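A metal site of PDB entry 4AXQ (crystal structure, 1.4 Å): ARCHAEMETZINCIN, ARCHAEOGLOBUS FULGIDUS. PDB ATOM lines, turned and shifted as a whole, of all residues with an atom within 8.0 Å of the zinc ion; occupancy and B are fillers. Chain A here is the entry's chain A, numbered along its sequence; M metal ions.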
ATOM      1  N   GLY A  86      -4.962  36.580  23.969  1.00  0.00           N
ATOM      2  CA  GLY A  86      -5.608  36.106  22.762  1.00  0.00           C
ATOM      3  C   GLY A  86      -7.114  36.143  22.896  1.00  0.00           C
ATOM      4  O   GLY A  86      -7.641  36.573  23.921  1.00  0.00           O
ATOM      5  N   GLU A  87      -7.781  35.676  21.857  1.00  0.00           N
ATOM      6  CA  GLU A  87      -9.238  35.636  21.787  1.00  0.00           C
ATOM      7  C   GLU A  87      -9.619  34.580  20.779  1.00  0.00           C
ATOM      8  O   GLU A  87      -8.883  34.349  19.833  1.00  0.00           O
ATOM      9  CB  GLU A  87      -9.831  37.020  21.428  1.00  0.00           C
ATOM     10  CG  GLU A  87     -11.372  37.028  21.534  1.00  0.00           C
ATOM     11  CD  GLU A  87     -11.999  38.412  21.445  1.00  0.00           C
ATOM     12  OE1 GLU A  87     -11.322  39.381  21.071  1.00  0.00           O
ATOM     13  OE2 GLU A  87     -13.211  38.525  21.759  1.00  0.00           O
ATOM     14  N   ALA A  88     -10.788  33.969  20.973  1.00  0.00           N
ATOM     15  CA  ALA A  88     -11.227  32.887  20.114  1.00  0.00           C
ATOM     16  C   ALA A  88     -12.714  32.963  19.878  1.00  0.00           C
ATOM     17  O   ALA A  88     -13.462  33.447  20.719  1.00  0.00           O
ATOM     18  CB  ALA A  88     -10.927  31.546  20.759  1.00  0.00           C
ATOM     19  N   GLU A 117      -0.687  28.883  25.322  1.00  0.00           N
ATOM     20  CA  GLU A 117      -1.728  29.806  24.934  1.00  0.00           C
ATOM     21  C   GLU A 117      -2.338  29.471  23.570  1.00  0.00           C
ATOM     22  O   GLU A 117      -3.543  29.637  23.391  1.00  0.00           O
ATOM     23  CB  GLU A 117      -1.246  31.255  25.045  1.00  0.00           C
ATOM     24  CG  GLU A 117      -1.226  31.720  26.490  1.00  0.00           C
ATOM     25  CD  GLU A 117      -2.603  31.624  27.137  1.00  0.00           C
ATOM     26  OE1 GLU A 117      -3.533  32.285  26.622  1.00  0.00           O
ATOM     27  OE2 GLU A 117      -2.768  30.845  28.112  1.00  0.00           O
ATOM     28  N   HIS A 120      -4.734  26.598  24.265  1.00  0.00           N
ATOM     29  CA  HIS A 120      -5.903  27.121  24.957  1.00  0.00           C
ATOM     30  C   HIS A 120      -6.868  27.778  23.964  1.00  0.00           C
ATOM     31  O   HIS A 120      -8.056  27.512  24.002  1.00  0.00           O
ATOM     32  CB  HIS A 120      -5.421  28.120  26.018  1.00  0.00           C
ATOM     33  CG  HIS A 120      -6.505  28.773  26.809  1.00  0.00           C
ATOM     34  ND1 HIS A 120      -6.911  28.321  28.037  1.00  0.00           N
ATOM     35  CD2 HIS A 120      -7.256  29.859  26.535  1.00  0.00           C
ATOM     36  CE1 HIS A 120      -7.883  29.103  28.484  1.00  0.00           C
ATOM     37  NE2 HIS A 120      -8.119  30.041  27.591  1.00  0.00           N
ATOM     38  N   GLU A 121      -6.374  28.664  23.113  1.00  0.00           N
ATOM     39  CA  GLU A 121      -7.251  29.342  22.166  1.00  0.00           C
ATOM     40  C   GLU A 121      -7.890  28.359  21.174  1.00  0.00           C
ATOM     41  O   GLU A 121      -9.067  28.457  20.847  1.00  0.00           O
ATOM     42  CB  GLU A 121      -6.523  30.466  21.412  1.00  0.00           C
ATOM     43  CG  GLU A 121      -5.971  31.570  22.273  1.00  0.00           C
ATOM     44  CD  GLU A 121      -6.993  32.299  23.149  1.00  0.00           C
ATOM     45  OE1 GLU A 121      -8.205  32.108  23.002  1.00  0.00           O
ATOM     46  OE2 GLU A 121      -6.557  33.115  24.008  1.00  0.00           O
ATOM     47  N   HIS A 124     -10.695  26.594  22.792  1.00  0.00           N
ATOM     48  CA  HIS A 124     -11.916  27.388  22.717  1.00  0.00           C
ATOM     49  C   HIS A 124     -12.589  27.255  21.348  1.00  0.00           C
ATOM     50  O   HIS A 124     -13.802  27.135  21.250  1.00  0.00           O
ATOM     51  CB  HIS A 124     -11.631  28.871  22.936  1.00  0.00           C
ATOM     52  CG  HIS A 124     -11.421  29.307  24.360  1.00  0.00           C
ATOM     53  ND1 HIS A 124     -12.249  28.958  25.395  1.00  0.00           N
ATOM     54  CD2 HIS A 124     -10.496  30.131  24.901  1.00  0.00           C
ATOM     55  CE1 HIS A 124     -11.839  29.535  26.512  1.00  0.00           C
ATOM     56  NE2 HIS A 124     -10.784  30.280  26.229  1.00  0.00           N
ATOM     57  N   LEU A 128     -14.425  24.254  23.737  1.00  0.00           N
ATOM     58  CA  LEU A 128     -14.138  24.070  25.165  1.00  0.00           C
ATOM     59  C   LEU A 128     -14.279  25.362  25.939  1.00  0.00           C
ATOM     60  O   LEU A 128     -13.710  26.370  25.563  1.00  0.00           O
ATOM     61  CB  LEU A 128     -12.742  23.522  25.389  1.00  0.00           C
ATOM     62  CG  LEU A 128     -12.461  22.138  24.799  1.00  0.00           C
ATOM     63  CD1 LEU A 128     -11.001  21.766  25.026  1.00  0.00           C
ATOM     64  CD2 LEU A 128     -13.384  21.083  25.380  1.00  0.00           C
ATOM     65  N   LYS A 129     -15.033  25.312  27.023  1.00  0.00           N
ATOM     66  CA  LYS A 129     -15.099  26.405  27.981  1.00  0.00           C
ATOM     67  C   LYS A 129     -13.915  26.339  28.955  1.00  0.00           C
ATOM     68  O   LYS A 129     -13.157  25.363  28.974  1.00  0.00           O
ATOM     69  CB  LYS A 129     -16.415  26.316  28.763  1.00  0.00           C
ATOM     70  CG  LYS A 129     -17.649  26.379  27.849  1.00  0.00           C
ATOM     71  CD  LYS A 129     -18.943  26.236  28.663  1.00  0.00           C
ATOM     72  CE  LYS A 129     -20.187  26.381  27.790  1.00  0.00           C
ATOM     73  NZ  LYS A 129     -20.331  25.257  26.805  1.00  0.00           N
ATOM     74  N   HIS A 130     -13.738  27.374  29.761  1.00  0.00           N
ATOM     75  CA  HIS A 130     -12.726  27.319  30.792  1.00  0.00           C
ATOM     76  C   HIS A 130     -12.994  26.171  31.755  1.00  0.00           C
ATOM     77  O   HIS A 130     -14.143  25.814  32.002  1.00  0.00           O
ATOM     78  CB  HIS A 130     -12.599  28.645  31.522  1.00  0.00           C
ATOM     79  CG  HIS A 130     -11.916  29.694  30.709  1.00  0.00           C
ATOM     80  ND1 HIS A 130     -12.079  31.037  30.946  1.00  0.00           N
ATOM     81  CD2 HIS A 130     -11.038  29.595  29.677  1.00  0.00           C
ATOM     82  CE1 HIS A 130     -11.353  31.728  30.086  1.00  0.00           C
ATOM     83  NE2 HIS A 130     -10.720  30.872  29.297  1.00  0.00           N
ATOM     84  N   CYS A 131     -11.919  25.626  32.301  1.00  0.00           N
ATOM     85  CA  CYS A 131     -11.961  24.376  33.038  1.00  0.00           C
ATOM     86  C   CYS A 131     -11.374  24.643  34.415  1.00  0.00           C
ATOM     87  O   CYS A 131     -10.470  25.472  34.536  1.00  0.00           O
ATOM     88  CB  CYS A 131     -11.104  23.350  32.287  1.00  0.00           C
ATOM     89  SG  CYS A 131     -11.045  21.726  33.046  1.00  0.00           S
ATOM     90  N   VAL A 136      -4.969  22.889  30.605  1.00  0.00           N
ATOM     91  CA  VAL A 136      -4.583  24.024  29.800  1.00  0.00           C
ATOM     92  C   VAL A 136      -5.777  24.977  29.567  1.00  0.00           C
ATOM     93  O   VAL A 136      -5.594  26.145  29.238  1.00  0.00           O
ATOM     94  CB  VAL A 136      -4.025  23.527  28.442  1.00  0.00           C
ATOM     95  CG1 VAL A 136      -5.099  22.867  27.593  1.00  0.00           C
ATOM     96  CG2 VAL A 136      -3.308  24.631  27.709  1.00  0.00           C
ATOM     97  N   MET A 137      -6.994  24.478  29.767  1.00  0.00           N
ATOM     98  CA  MET A 137      -8.169  25.317  29.597  1.00  0.00           C
ATOM     99  C   MET A 137      -8.495  26.152  30.827  1.00  0.00           C
ATOM    100  O   MET A 137      -9.498  26.850  30.827  1.00  0.00           O
ATOM    101  CB  MET A 137      -9.395  24.504  29.152  1.00  0.00           C
ATOM    102  CG  MET A 137      -9.267  23.915  27.751  1.00  0.00           C
ATOM    103  SD  MET A 137      -8.803  25.121  26.474  1.00  0.00           S
ATOM    104  CE  MET A 137     -10.065  26.400  26.661  1.00  0.00           C
ATOM    105  N   ARG A 138      -7.646  26.100  31.840  1.00  0.00           N
ATOM    106  CA  ARG A 138      -7.782  27.039  32.955  1.00  0.00           C
ATOM    107  C   ARG A 138      -7.657  28.459  32.398  1.00  0.00           C
ATOM    108  O   ARG A 138      -6.852  28.695  31.492  1.00  0.00           O
ATOM    109  CB  ARG A 138      -6.695  26.812  34.008  1.00  0.00           C
ATOM    110  CG  ARG A 138      -7.032  25.787  35.080  1.00  0.00           C
ATOM    111  CD  ARG A 138      -6.143  25.982  36.321  1.00  0.00           C
ATOM    112  NE  ARG A 138      -6.351  24.953  37.336  1.00  0.00           N
ATOM    113  CZ  ARG A 138      -7.372  24.930  38.189  1.00  0.00           C
ATOM    114  NH1 ARG A 138      -8.298  25.872  38.160  1.00  0.00           N
ATOM    115  NH2 ARG A 138      -7.466  23.951  39.074  1.00  0.00           N
ATOM    116  N   PHE A 139      -8.431  29.388  32.929  1.00  0.00           N
ATOM    117  CA  PHE A 139      -8.340  30.786  32.521  1.00  0.00           C
ATOM    118  C   PHE A 139      -6.945  31.323  32.826  1.00  0.00           C
ATOM    119  O   PHE A 139      -6.371  30.984  33.849  1.00  0.00           O
ATOM    120  CB  PHE A 139      -9.385  31.629  33.275  1.00  0.00           C
ATOM    121  CG  PHE A 139      -9.228  31.570  34.768  1.00  0.00           C
ATOM    122  CD1 PHE A 139      -9.850  30.571  35.499  1.00  0.00           C
ATOM    123  CD2 PHE A 139      -8.462  32.504  35.433  1.00  0.00           C
ATOM    124  CE1 PHE A 139      -9.719  30.508  36.877  1.00  0.00           C
ATOM    125  CE2 PHE A 139      -8.320  32.450  36.810  1.00  0.00           C
ATOM    126  CZ  PHE A 139      -8.946  31.456  37.529  1.00  0.00           C
ATOM    127  N   SER A 140      -6.386  32.130  31.934  1.00  0.00           N
ATOM    128  CA  SER A 140      -5.136  32.812  32.214  1.00  0.00           C
ATOM    129  C   SER A 140      -5.197  34.278  31.811  1.00  0.00           C
ATOM    130  O   SER A 140      -5.463  34.605  30.651  1.00  0.00           O
ATOM    131  CB  SER A 140      -3.960  32.137  31.503  1.00  0.00           C
ATOM    132  OG  SER A 140      -3.575  30.927  32.164  1.00  0.00           O
ATOM    133  N   ASN A 141      -4.967  35.148  32.778  1.00  0.00           N
ATOM    134  CA  ASN A 141      -4.892  36.579  32.522  1.00  0.00           C
ATOM    135  C   ASN A 141      -3.542  37.178  32.933  1.00  0.00           C
ATOM    136  O   ASN A 141      -3.286  38.355  32.675  1.00  0.00           O
ATOM    137  CB  ASN A 141      -6.037  37.305  33.237  1.00  0.00           C
ATOM    138  CG  ASN A 141      -7.395  36.899  32.711  1.00  0.00           C
ATOM    139  OD1 ASN A 141      -7.756  37.197  31.566  1.00  0.00           O
ATOM    140  ND2 ASN A 141      -8.176  36.216  33.552  1.00  0.00           N
ATOM    141  N   LYS A 149      -0.380  26.390  35.007  1.00  0.00           N
ATOM    142  CA  LYS A 149      -1.260  25.378  34.417  1.00  0.00           C
ATOM    143  C   LYS A 149      -0.445  24.513  33.478  1.00  0.00           C
ATOM    144  O   LYS A 149       0.608  24.938  33.003  1.00  0.00           O
ATOM    145  CB  LYS A 149      -2.426  26.021  33.674  1.00  0.00           C
ATOM    146  CG  LYS A 149      -2.079  26.650  32.334  1.00  0.00           C
ATOM    147  CD  LYS A 149      -3.293  27.393  31.831  1.00  0.00           C
ATOM    148  CE  LYS A 149      -3.064  28.065  30.517  1.00  0.00           C
ATOM    149  NZ  LYS A 149      -4.235  28.928  30.200  1.00  0.00           N
HETATM  150 ZN    ZN M   1      -9.648  31.495  27.609  1.00  0.00          ZN
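The nearest printed residue that does not touch the zinc ion is Glu 121 (4.9 Å).
The zinc ion is bound by a ring nitrogen (NE2) of His 130 (2.1 Å), a ring nitrogen (NE2) of His 120 (2.1 Å) and a ring nitrogen (NE2) of His 124 (2.2 Å). The zinc ion has three donor atoms within binding distance.
The backbone carbonyl oxygen (O) of Arg 138 lies close to a ring nitrogen (ND1) of His 120, at 3.5 Å. The backbone carbonyl oxygen (O) of Val 136 lies within hydrogen-bond range of a ring nitrogen (ND1) of His 120 (2.8 Å). A ring nitrogen (ND1) of His 120 lies within hydrogen-bond range of the side-chain amino group (NZ) of Lys 149. A ring nitrogen (ND1) of His 124 sits at hydrogen-bond distance from the backbone carbonyl oxygen (O) of Leu 128 (3.0 Å).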
